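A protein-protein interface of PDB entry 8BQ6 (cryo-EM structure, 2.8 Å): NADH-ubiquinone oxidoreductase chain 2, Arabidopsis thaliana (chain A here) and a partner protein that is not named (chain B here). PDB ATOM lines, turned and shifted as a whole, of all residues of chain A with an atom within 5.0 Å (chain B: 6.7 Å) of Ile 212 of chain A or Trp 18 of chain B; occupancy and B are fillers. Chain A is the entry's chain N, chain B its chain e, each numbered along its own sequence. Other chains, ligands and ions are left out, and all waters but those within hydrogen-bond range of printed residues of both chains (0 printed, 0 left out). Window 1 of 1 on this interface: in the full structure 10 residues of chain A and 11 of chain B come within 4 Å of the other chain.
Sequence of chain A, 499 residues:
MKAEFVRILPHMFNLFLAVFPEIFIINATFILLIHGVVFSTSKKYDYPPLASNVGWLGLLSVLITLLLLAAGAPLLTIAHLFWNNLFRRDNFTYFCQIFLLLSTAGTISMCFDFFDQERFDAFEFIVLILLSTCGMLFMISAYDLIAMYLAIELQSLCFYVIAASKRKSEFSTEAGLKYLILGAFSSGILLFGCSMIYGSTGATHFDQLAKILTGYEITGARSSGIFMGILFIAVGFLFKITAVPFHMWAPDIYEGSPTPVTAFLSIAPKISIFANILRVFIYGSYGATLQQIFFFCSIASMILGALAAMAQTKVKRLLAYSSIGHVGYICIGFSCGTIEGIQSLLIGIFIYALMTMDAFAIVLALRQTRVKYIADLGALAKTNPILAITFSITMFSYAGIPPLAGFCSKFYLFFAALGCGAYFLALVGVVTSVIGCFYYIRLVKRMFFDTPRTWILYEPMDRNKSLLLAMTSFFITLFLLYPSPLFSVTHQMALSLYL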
ATOM      1  N   THR A 201       3.406   2.295 -14.463  1.00  0.00           N
ATOM      2  CA  THR A 201       3.494   3.749 -14.489  1.00  0.00           C
ATOM      3  C   THR A 201       3.470   4.404 -13.116  1.00  0.00           C
ATOM      4  O   THR A 201       3.737   5.608 -13.025  1.00  0.00           O
ATOM      5  CB  THR A 201       2.359   4.337 -15.339  1.00  0.00           C
ATOM      6  OG1 THR A 201       1.110   4.161 -14.659  1.00  0.00           O
ATOM      7  CG2 THR A 201       2.296   3.675 -16.703  1.00  0.00           C
ATOM      8  N   ALA A 203       0.916   5.141 -11.591  1.00  0.00           N
ATOM      9  CA  ALA A 203      -0.180   6.131 -11.655  1.00  0.00           C
ATOM     10  C   ALA A 203      -1.539   5.494 -11.950  1.00  0.00           C
ATOM     11  O   ALA A 203      -1.597   4.575 -12.785  1.00  0.00           O
ATOM     12  CB  ALA A 203       0.156   7.140 -12.711  1.00  0.00           C
ATOM     13  N   GLN A 208      -2.518  11.675 -15.096  1.00  0.00           N
ATOM     14  CA  GLN A 208      -1.132  11.172 -14.961  1.00  0.00           C
ATOM     15  C   GLN A 208      -0.885  10.143 -16.065  1.00  0.00           C
ATOM     16  O   GLN A 208       0.148  10.243 -16.722  1.00  0.00           O
ATOM     17  CB  GLN A 208      -0.931  10.605 -13.557  1.00  0.00           C
ATOM     18  CG  GLN A 208      -1.396  11.516 -12.434  1.00  0.00           C
ATOM     19  CD  GLN A 208      -1.349  10.829 -11.091  1.00  0.00           C
ATOM     20  OE1 GLN A 208      -1.543   9.621 -10.977  1.00  0.00           O
ATOM     21  NE2 GLN A 208      -1.101  11.601 -10.049  1.00  0.00           N
ATOM     22  N   LEU A 209      -1.824   9.221 -16.281  1.00  0.00           N
ATOM     23  CA  LEU A 209      -1.685   8.227 -17.338  1.00  0.00           C
ATOM     24  C   LEU A 209      -1.579   8.890 -18.700  1.00  0.00           C
ATOM     25  O   LEU A 209      -0.846   8.418 -19.575  1.00  0.00           O
ATOM     26  CB  LEU A 209      -2.872   7.271 -17.317  1.00  0.00           C
ATOM     27  CG  LEU A 209      -3.026   6.372 -16.099  1.00  0.00           C
ATOM     28  CD1 LEU A 209      -4.293   5.552 -16.231  1.00  0.00           C
ATOM     29  CD2 LEU A 209      -1.820   5.480 -15.978  1.00  0.00           C
ATOM     30  N   ALA A 210      -2.325   9.975 -18.907  1.00  0.00           N
ATOM     31  CA  ALA A 210      -2.205  10.719 -20.153  1.00  0.00           C
ATOM     32  C   ALA A 210      -0.790  11.249 -20.330  1.00  0.00           C
ATOM     33  O   ALA A 210      -0.153  11.017 -21.360  1.00  0.00           O
ATOM     34  CB  ALA A 210      -3.225  11.857 -20.181  1.00  0.00           C
ATOM     35  N   LYS A 211      -0.256  11.920 -19.311  1.00  0.00           N
ATOM     36  CA  LYS A 211       1.075  12.506 -19.449  1.00  0.00           C
ATOM     37  C   LYS A 211       2.145  11.441 -19.663  1.00  0.00           C
ATOM     38  O   LYS A 211       3.067  11.631 -20.464  1.00  0.00           O
ATOM     39  CB  LYS A 211       1.398  13.354 -18.228  1.00  0.00           C
ATOM     40  CG  LYS A 211       0.752  14.707 -18.275  1.00  0.00           C
ATOM     41  CD  LYS A 211       0.966  15.441 -16.984  1.00  0.00           C
ATOM     42  CE  LYS A 211       0.700  16.915 -17.165  1.00  0.00           C
ATOM     43  NZ  LYS A 211      -0.755  17.205 -17.205  1.00  0.00           N
ATOM     44  N   ILE A 212       2.040  10.315 -18.954  1.00  0.00           N
ATOM     45  CA  ILE A 212       3.057   9.270 -19.049  1.00  0.00           C
ATOM     46  C   ILE A 212       3.054   8.640 -20.438  1.00  0.00           C
ATOM     47  O   ILE A 212       4.111   8.331 -21.001  1.00  0.00           O
ATOM     48  CB  ILE A 212       2.836   8.203 -17.962  1.00  0.00           C
ATOM     49  CG1 ILE A 212       3.244   8.723 -16.594  1.00  0.00           C
ATOM     50  CG2 ILE A 212       3.645   6.960 -18.254  1.00  0.00           C
ATOM     51  CD1 ILE A 212       2.433   8.120 -15.471  1.00  0.00           C
ATOM     52  N   LEU A 213       1.868   8.438 -21.011  1.00  0.00           N
ATOM     53  CA  LEU A 213       1.754   7.591 -22.191  1.00  0.00           C
ATOM     54  C   LEU A 213       1.753   8.352 -23.513  1.00  0.00           C
ATOM     55  O   LEU A 213       1.937   7.722 -24.560  1.00  0.00           O
ATOM     56  CB  LEU A 213       0.489   6.739 -22.103  1.00  0.00           C
ATOM     57  CG  LEU A 213       0.246   5.754 -20.960  1.00  0.00           C
ATOM     58  CD1 LEU A 213      -0.859   4.795 -21.353  1.00  0.00           C
ATOM     59  CD2 LEU A 213       1.503   4.989 -20.626  1.00  0.00           C
ATOM     60  N   THR A 214       1.544   9.668 -23.514  1.00  0.00           N
ATOM     61  CA  THR A 214       1.544  10.407 -24.772  1.00  0.00           C
ATOM     62  C   THR A 214       2.952  10.653 -25.292  1.00  0.00           C
ATOM     63  O   THR A 214       3.894  10.859 -24.523  1.00  0.00           O
ATOM     64  CB  THR A 214       0.831  11.749 -24.638  1.00  0.00           C
ATOM     65  OG1 THR A 214       1.586  12.642 -23.804  1.00  0.00           O
ATOM     66  CG2 THR A 214      -0.609  11.600 -24.159  1.00  0.00           C
ATOM     67  N   TYR A 216       4.737   8.507 -27.075  1.00  0.00           N
ATOM     68  CA  TYR A 216       5.615   7.354 -27.207  1.00  0.00           C
ATOM     69  C   TYR A 216       4.956   6.167 -27.888  1.00  0.00           C
ATOM     70  O   TYR A 216       5.572   5.565 -28.773  1.00  0.00           O
ATOM     71  CB  TYR A 216       6.131   6.980 -25.812  1.00  0.00           C
ATOM     72  CG  TYR A 216       7.130   7.995 -25.321  1.00  0.00           C
ATOM     73  CD1 TYR A 216       6.706   9.163 -24.701  1.00  0.00           C
ATOM     74  CD2 TYR A 216       8.492   7.808 -25.505  1.00  0.00           C
ATOM     75  CE1 TYR A 216       7.606  10.109 -24.274  1.00  0.00           C
ATOM     76  CE2 TYR A 216       9.404   8.747 -25.072  1.00  0.00           C
ATOM     77  CZ  TYR A 216       8.955   9.895 -24.455  1.00  0.00           C
ATOM     78  OH  TYR A 216       9.857  10.837 -24.020  1.00  0.00           O
ATOM     79  N   ILE A 226       2.414  -1.890 -19.548  1.00  0.00           N
ATOM     80  CA  ILE A 226       1.384  -0.944 -19.972  1.00  0.00           C
ATOM     81  C   ILE A 226       0.522  -1.556 -21.064  1.00  0.00           C
ATOM     82  O   ILE A 226      -0.714  -1.465 -21.036  1.00  0.00           O
ATOM     83  CB  ILE A 226       2.039   0.363 -20.455  1.00  0.00           C
ATOM     84  CG1 ILE A 226       2.755   1.069 -19.310  1.00  0.00           C
ATOM     85  CG2 ILE A 226       1.007   1.284 -21.069  1.00  0.00           C
ATOM     86  CD1 ILE A 226       3.582   2.237 -19.767  1.00  0.00           C
ATOM     87  N   MET B   1       4.658   6.008  -8.463  1.00  0.00           N
ATOM     88  CA  MET B   1       4.875   7.031  -7.417  1.00  0.00           C
ATOM     89  C   MET B   1       4.589   8.411  -8.007  1.00  0.00           C
ATOM     90  O   MET B   1       5.532   9.205  -8.148  1.00  0.00           O
ATOM     91  CB  MET B   1       6.312   6.958  -6.902  1.00  0.00           C
ATOM     92  CG  MET B   1       6.658   7.981  -5.839  1.00  0.00           C
ATOM     93  SD  MET B   1       5.796   7.743  -4.279  1.00  0.00           S
ATOM     94  CE  MET B   1       6.485   9.142  -3.421  1.00  0.00           C
ATOM     95  N   ALA B   2       3.331   8.671  -8.351  1.00  0.00           N
ATOM     96  CA  ALA B   2       2.933   9.987  -8.894  1.00  0.00           C
ATOM     97  C   ALA B   2       2.020  10.705  -7.900  1.00  0.00           C
ATOM     98  O   ALA B   2       1.792  11.899  -8.096  1.00  0.00           O
ATOM     99  CB  ALA B   2       2.248   9.796 -10.219  1.00  0.00           C
ATOM    100  N   SER B   3       1.517  10.003  -6.881  1.00  0.00           N
ATOM    101  CA  SER B   3       0.539  10.604  -5.936  1.00  0.00           C
ATOM    102  C   SER B   3       1.235  11.446  -4.867  1.00  0.00           C
ATOM    103  O   SER B   3       0.628  12.415  -4.431  1.00  0.00           O
ATOM    104  CB  SER B   3      -0.344   9.550  -5.322  1.00  0.00           C
ATOM    105  OG  SER B   3       0.244   8.973  -4.165  1.00  0.00           O
ATOM    106  N   GLY B   4       2.439  11.062  -4.449  1.00  0.00           N
ATOM    107  CA  GLY B   4       3.170  11.810  -3.410  1.00  0.00           C
ATOM    108  C   GLY B   4       3.129  11.143  -2.055  1.00  0.00           C
ATOM    109  O   GLY B   4       4.002  11.442  -1.234  1.00  0.00           O
ATOM    110  N   CYS B  14       9.784   8.690  -5.630  1.00  0.00           N
ATOM    111  CA  CYS B  14       9.827   9.129  -7.017  1.00  0.00           C
ATOM    112  C   CYS B  14       8.889  10.293  -7.311  1.00  0.00           C
ATOM    113  O   CYS B  14       8.578  10.545  -8.479  1.00  0.00           O
ATOM    114  CB  CYS B  14       9.513   7.954  -7.942  1.00  0.00           C
ATOM    115  SG  CYS B  14      10.638   6.549  -7.745  1.00  0.00           S
ATOM    116  N   TYR B  15       8.423  10.999  -6.282  1.00  0.00           N
ATOM    117  CA  TYR B  15       7.439  12.094  -6.473  1.00  0.00           C
ATOM    118  C   TYR B  15       8.105  13.312  -7.110  1.00  0.00           C
ATOM    119  O   TYR B  15       7.499  13.918  -7.990  1.00  0.00           O
ATOM    120  CB  TYR B  15       6.842  12.513  -5.134  1.00  0.00           C
ATOM    121  CG  TYR B  15       5.865  13.654  -5.188  1.00  0.00           C
ATOM    122  CD1 TYR B  15       4.717  13.591  -5.960  1.00  0.00           C
ATOM    123  CD2 TYR B  15       6.095  14.800  -4.450  1.00  0.00           C
ATOM    124  CE1 TYR B  15       3.818  14.642  -5.989  1.00  0.00           C
ATOM    125  CE2 TYR B  15       5.213  15.861  -4.469  1.00  0.00           C
ATOM    126  CZ  TYR B  15       4.073  15.778  -5.242  1.00  0.00           C
ATOM    127  OH  TYR B  15       3.219  16.836  -5.247  1.00  0.00           O
ATOM    128  N   ASP B  16       9.305  13.660  -6.656  1.00  0.00           N
ATOM    129  CA  ASP B  16       9.963  14.847  -7.195  1.00  0.00           C
ATOM    130  C   ASP B  16      10.255  14.697  -8.684  1.00  0.00           C
ATOM    131  O   ASP B  16      10.099  15.654  -9.453  1.00  0.00           O
ATOM    132  CB  ASP B  16      11.244  15.134  -6.417  1.00  0.00           C
ATOM    133  CG  ASP B  16      10.969  15.737  -5.054  1.00  0.00           C
ATOM    134  OD1 ASP B  16       9.856  16.263  -4.851  1.00  0.00           O
ATOM    135  OD2 ASP B  16      11.857  15.678  -4.180  1.00  0.00           O
ATOM    136  N   PHE B  17      10.674  13.503  -9.111  1.00  0.00           N
ATOM    137  CA  PHE B  17      10.868  13.250 -10.536  1.00  0.00           C
ATOM    138  C   PHE B  17       9.558  13.384 -11.297  1.00  0.00           C
ATOM    139  O   PHE B  17       9.515  13.946 -12.402  1.00  0.00           O
ATOM    140  CB  PHE B  17      11.459  11.857 -10.753  1.00  0.00           C
ATOM    141  CG  PHE B  17      12.917  11.750 -10.419  1.00  0.00           C
ATOM    142  CD1 PHE B  17      13.866  12.378 -11.205  1.00  0.00           C
ATOM    143  CD2 PHE B  17      13.342  10.986  -9.346  1.00  0.00           C
ATOM    144  CE1 PHE B  17      15.208  12.272 -10.909  1.00  0.00           C
ATOM    145  CE2 PHE B  17      14.685  10.873  -9.050  1.00  0.00           C
ATOM    146  CZ  PHE B  17      15.618  11.518  -9.831  1.00  0.00           C
ATOM    147  N   TRP B  18       8.483  12.833 -10.729  1.00  0.00           N
ATOM    148  CA  TRP B  18       7.150  12.945 -11.371  1.00  0.00           C
ATOM    149  C   TRP B  18       6.789  14.420 -11.530  1.00  0.00           C
ATOM    150  O   TRP B  18       6.351  14.798 -12.615  1.00  0.00           O
ATOM    151  CB  TRP B  18       6.072  12.211 -10.562  1.00  0.00           C
ATOM    152  CG  TRP B  18       4.702  12.574 -11.034  1.00  0.00           C
ATOM    153  CD1 TRP B  18       3.775  13.337 -10.390  1.00  0.00           C
ATOM    154  CD2 TRP B  18       4.138  12.248 -12.314  1.00  0.00           C
ATOM    155  NE1 TRP B  18       2.663  13.486 -11.170  1.00  0.00           N
ATOM    156  CE2 TRP B  18       2.855  12.828 -12.354  1.00  0.00           C
ATOM    157  CE3 TRP B  18       4.585  11.515 -13.416  1.00  0.00           C
ATOM    158  CZ2 TRP B  18       2.016  12.693 -13.456  1.00  0.00           C
ATOM    159  CZ3 TRP B  18       3.757  11.390 -14.504  1.00  0.00           C
ATOM    160  CH2 TRP B  18       2.490  11.968 -14.523  1.00  0.00           C
ATOM    161  N   MET B  19       6.964  15.206 -10.468  1.00  0.00           N
ATOM    162  CA  MET B  19       6.581  16.610 -10.520  1.00  0.00           C
ATOM    163  C   MET B  19       7.431  17.385 -11.519  1.00  0.00           C
ATOM    164  O   MET B  19       6.920  18.270 -12.212  1.00  0.00           O
ATOM    165  CB  MET B  19       6.667  17.232  -9.130  1.00  0.00           C
ATOM    166  CG  MET B  19       5.519  16.832  -8.234  1.00  0.00           C
ATOM    167  SD  MET B  19       3.967  16.755  -9.152  1.00  0.00           S
ATOM    168  CE  MET B  19       3.021  18.029  -8.327  1.00  0.00           C
ATOM    169  N   ASP B  20       8.725  17.069 -11.615  1.00  0.00           N
ATOM    170  CA  ASP B  20       9.553  17.692 -12.647  1.00  0.00           C
ATOM    171  C   ASP B  20       9.021  17.374 -14.038  1.00  0.00           C
ATOM    172  O   ASP B  20       8.875  18.268 -14.883  1.00  0.00           O
ATOM    173  CB  ASP B  20      11.000  17.225 -12.522  1.00  0.00           C
ATOM    174  CG  ASP B  20      11.636  17.654 -11.228  1.00  0.00           C
ATOM    175  OD1 ASP B  20      12.674  17.071 -10.859  1.00  0.00           O
ATOM    176  OD2 ASP B  20      11.103  18.581 -10.584  1.00  0.00           O
ATOM    177  N   PHE B  21       8.718  16.100 -14.289  1.00  0.00           N
ATOM    178  CA  PHE B  21       8.211  15.711 -15.599  1.00  0.00           C
ATOM    179  C   PHE B  21       6.879  16.391 -15.903  1.00  0.00           C
ATOM    180  O   PHE B  21       6.651  16.861 -17.025  1.00  0.00           O
ATOM    181  CB  PHE B  21       8.077  14.192 -15.661  1.00  0.00           C
ATOM    182  CG  PHE B  21       7.356  13.692 -16.871  1.00  0.00           C
ATOM    183  CD1 PHE B  21       7.852  13.927 -18.134  1.00  0.00           C
ATOM    184  CD2 PHE B  21       6.183  12.973 -16.740  1.00  0.00           C
ATOM    185  CE1 PHE B  21       7.189  13.459 -19.245  1.00  0.00           C
ATOM    186  CE2 PHE B  21       5.518  12.504 -17.846  1.00  0.00           C
ATOM    187  CZ  PHE B  21       6.022  12.745 -19.099  1.00  0.00           C
ATOM    188  N   SER B  22       5.994  16.466 -14.908  1.00  0.00           N
ATOM    189  CA  SER B  22       4.687  17.081 -15.118  1.00  0.00           C
ATOM    190  C   SER B  22       4.813  18.572 -15.388  1.00  0.00           C
ATOM    191  O   SER B  22       4.164  19.104 -16.298  1.00  0.00           O
ATOM    192  CB  SER B  22       3.793  16.839 -13.904  1.00  0.00           C
ATOM    193  OG  SER B  22       3.517  15.461 -13.757  1.00  0.00           O
ATOM    194  N   GLU B  23       5.629  19.267 -14.597  1.00  0.00           N
ATOM    195  CA  GLU B  23       5.800  20.697 -14.804  1.00  0.00           C
ATOM    196  C   GLU B  23       6.419  20.976 -16.168  1.00  0.00           C
ATOM    197  O   GLU B  23       6.024  21.929 -16.849  1.00  0.00           O
ATOM    198  CB  GLU B  23       6.644  21.295 -13.676  1.00  0.00           C
ATOM    199  CG  GLU B  23       5.953  21.362 -12.336  1.00  0.00           C
ATOM    200  CD  GLU B  23       6.789  21.988 -11.255  1.00  0.00           C
ATOM    201  OE1 GLU B  23       6.768  23.231 -11.149  1.00  0.00           O
ATOM    202  OE2 GLU B  23       7.464  21.248 -10.509  1.00  0.00           O
ATOM    203  N   MET B  25       5.975  19.058 -18.847  1.00  0.00           N
ATOM    204  CA  MET B  25       4.954  18.782 -19.856  1.00  0.00           C
ATOM    205  C   MET B  25       3.817  19.794 -19.852  1.00  0.00           C
ATOM    206  O   MET B  25       3.056  19.850 -20.823  1.00  0.00           O
ATOM    207  CB  MET B  25       4.363  17.385 -19.672  1.00  0.00           C
ATOM    208  CG  MET B  25       5.296  16.259 -20.039  1.00  0.00           C
ATOM    209  SD  MET B  25       4.937  15.509 -21.642  1.00  0.00           S
ATOM    210  CE  MET B  25       3.200  15.111 -21.487  1.00  0.00           C
ATOM    211  N   LEU B  37      13.361  13.962 -18.518  1.00  0.00           N
ATOM    212  CA  LEU B  37      12.666  13.919 -17.234  1.00  0.00           C
ATOM    213  C   LEU B  37      11.753  12.704 -17.136  1.00  0.00           C
ATOM    214  O   LEU B  37      11.621  12.094 -16.064  1.00  0.00           O
ATOM    215  CB  LEU B  37      11.876  15.211 -17.032  1.00  0.00           C
ATOM    216  CG  LEU B  37      12.709  16.477 -17.226  1.00  0.00           C
ATOM    217  CD1 LEU B  37      11.899  17.712 -16.913  1.00  0.00           C
ATOM    218  CD2 LEU B  37      13.934  16.413 -16.343  1.00  0.00           C
ATOM    219  N   ARG B  38      11.111  12.338 -18.246  1.00  0.00           N
ATOM    220  CA  ARG B  38      10.252  11.161 -18.237  1.00  0.00           C
ATOM    221  C   ARG B  38      11.048   9.900 -17.933  1.00  0.00           C
ATOM    222  O   ARG B  38      10.627   9.069 -17.114  1.00  0.00           O
ATOM    223  CB  ARG B  38       9.539  11.022 -19.575  1.00  0.00           C
ATOM    224  CG  ARG B  38       8.570   9.867 -19.626  1.00  0.00           C
ATOM    225  CD  ARG B  38       8.400   9.408 -21.048  1.00  0.00           C
ATOM    226  NE  ARG B  38       7.287   8.484 -21.207  1.00  0.00           N
ATOM    227  CZ  ARG B  38       7.417   7.206 -21.531  1.00  0.00           C
ATOM    228  NH1 ARG B  38       8.606   6.658 -21.720  1.00  0.00           N
ATOM    229  NH2 ARG B  38       6.326   6.458 -21.671  1.00  0.00           N
ATOM    230  N   TYR B  41      11.972   9.725 -14.287  1.00  0.00           N
ATOM    231  CA  TYR B  41      10.853   9.215 -13.454  1.00  0.00           C
ATOM    232  C   TYR B  41      10.768   7.690 -13.586  1.00  0.00           C
ATOM    233  O   TYR B  41      10.671   7.013 -12.561  1.00  0.00           O
ATOM    234  CB  TYR B  41       9.541   9.894 -13.859  1.00  0.00           C
ATOM    235  CG  TYR B  41       8.315   9.282 -13.233  1.00  0.00           C
ATOM    236  CD1 TYR B  41       8.110   9.345 -11.867  1.00  0.00           C
ATOM    237  CD2 TYR B  41       7.369   8.624 -14.002  1.00  0.00           C
ATOM    238  CE1 TYR B  41       6.994   8.778 -11.276  1.00  0.00           C
ATOM    239  CE2 TYR B  41       6.247   8.052 -13.428  1.00  0.00           C
ATOM    240  CZ  TYR B  41       6.056   8.135 -12.061  1.00  0.00           C
ATOM    241  OH  TYR B  41       4.956   7.579 -11.479  1.00  0.00           O
ATOM    242  N   LEU B  42      10.796   7.174 -14.817  1.00  0.00           N
ATOM    243  CA  LEU B  42      10.659   5.732 -15.004  1.00  0.00           C
ATOM    244  C   LEU B  42      11.866   4.971 -14.456  1.00  0.00           C
ATOM    245  O   LEU B  42      11.715   3.854 -13.935  1.00  0.00           O
ATOM    246  CB  LEU B  42      10.432   5.416 -16.478  1.00  0.00           C
ATOM    247  CG  LEU B  42       9.098   5.901 -17.053  1.00  0.00           C
ATOM    248  CD1 LEU B  42       9.012   5.569 -18.525  1.00  0.00           C
ATOM    249  CD2 LEU B  42       7.932   5.280 -16.306  1.00  0.00           C
ATOM    250  N   LEU B  45      11.280   4.606 -10.912  1.00  0.00           N
ATOM    251  CA  LEU B  45      10.300   3.558 -10.647  1.00  0.00           C
ATOM    252  C   LEU B  45      10.941   2.175 -10.669  1.00  0.00           C
ATOM    253  O   LEU B  45      10.747   1.385  -9.738  1.00  0.00           O
ATOM    254  CB  LEU B  45       9.155   3.621 -11.653  1.00  0.00           C
ATOM    255  CG  LEU B  45       8.139   4.764 -11.613  1.00  0.00           C
ATOM    256  CD1 LEU B  45       6.952   4.370 -12.456  1.00  0.00           C
ATOM    257  CD2 LEU B  45       7.694   5.122 -10.204  1.00  0.00           C
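The backbone carbonyl oxygen of Ile 212 of chain A lies within hydrogen-bond range of the guanidinium group of Arg 38 of chain B, 3.0 Å away. O of Thr 201 of chain A sits at hydrogen-bond distance from OH of Tyr 41 of chain B (2.8 Å).
Thr 201 of chain A touches Leu 45 of chain B (O to CD1, 3.5 Å). Gln 208 of chain A touches Ala 2 of chain B. Gln 208 of chain A touches Trp 18 of chain B (CB to CZ2, 3.6 Å). O of Lys 211 of chain A touches CZ of Phe 21 of chain B (3.4 Å). O of Lys 211 of chain A touches CE of Met 25 of chain B (3.6 Å). Trp 18 of chain B touches Ile 212 of chain A (CZ3 to CG1, 3.4 Å). Met 25 of chain B touches Thr 214 of chain A. CD of Arg 38 of chain B touches CE1 of Tyr 216 of chain A (3.4 Å).
The backbone carbonyl oxygen (O) of Ala 210 of chain A lies close to the side-chain hydroxyl (OG1) of Thr 214 of chain A, at 3.4 Å. N of Ala 203 of chain A sits close to OG1 of Thr 201 of chain A (3.2 Å). SG of Cys 14 of chain B is in hydrogen-bond range of N of Leu 45 of chain B, at 3.8 Å. N of Met 1 of chain B sits at hydrogen-bond distance from OH of Tyr 41 of chain B, 3.4 Å away. The side-chain hydroxyl (OG) of Ser 22 of chain B sits close to the backbone carbonyl oxygen (O) of Trp 18 of chain B, 3.1 Å away.
Hydrophobic or aromatic side chains of chain B within 4 Å of the printed part of chain A: Ala 2, Trp 18, Phe 21, Met 25, Tyr 41 and Leu 45. Along chain B the printed residues that touch a printed residue of chain A span positions 2 to 45. Hydrophobic or aromatic side chains of chain A within 4 Å of the printed part of chain B: Ile 212 and Tyr 216.
Printed residues of chain B within 4 Å of Lys 211 of chain A: Phe 21 (3.4 Å) and Met 25 (3.6 Å). Printed residues of chain B within 4 Å of Ile 212 of chain A: Trp 18 (3.4 Å) and Arg 38 (3.0 Å). Ile 226 of chain A touches none of the printed residues of chain B. Of chain A, only Gln 208 (3.6 Å) and Ile 212 (3.4 Å) come within 4 Å of Trp 18 of chain B. Printed residues of chain A within 4 Å of Met 25 of chain B: Lys 211 (3.6 Å) and Thr 214 (3.8 Å). Of the printed residues of chain A, Tyr 41 of chain B touches Thr 201. The nearest residue of chain B that does not touch Ile 212 of chain A is Phe 21 of chain B (4.2 Å).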
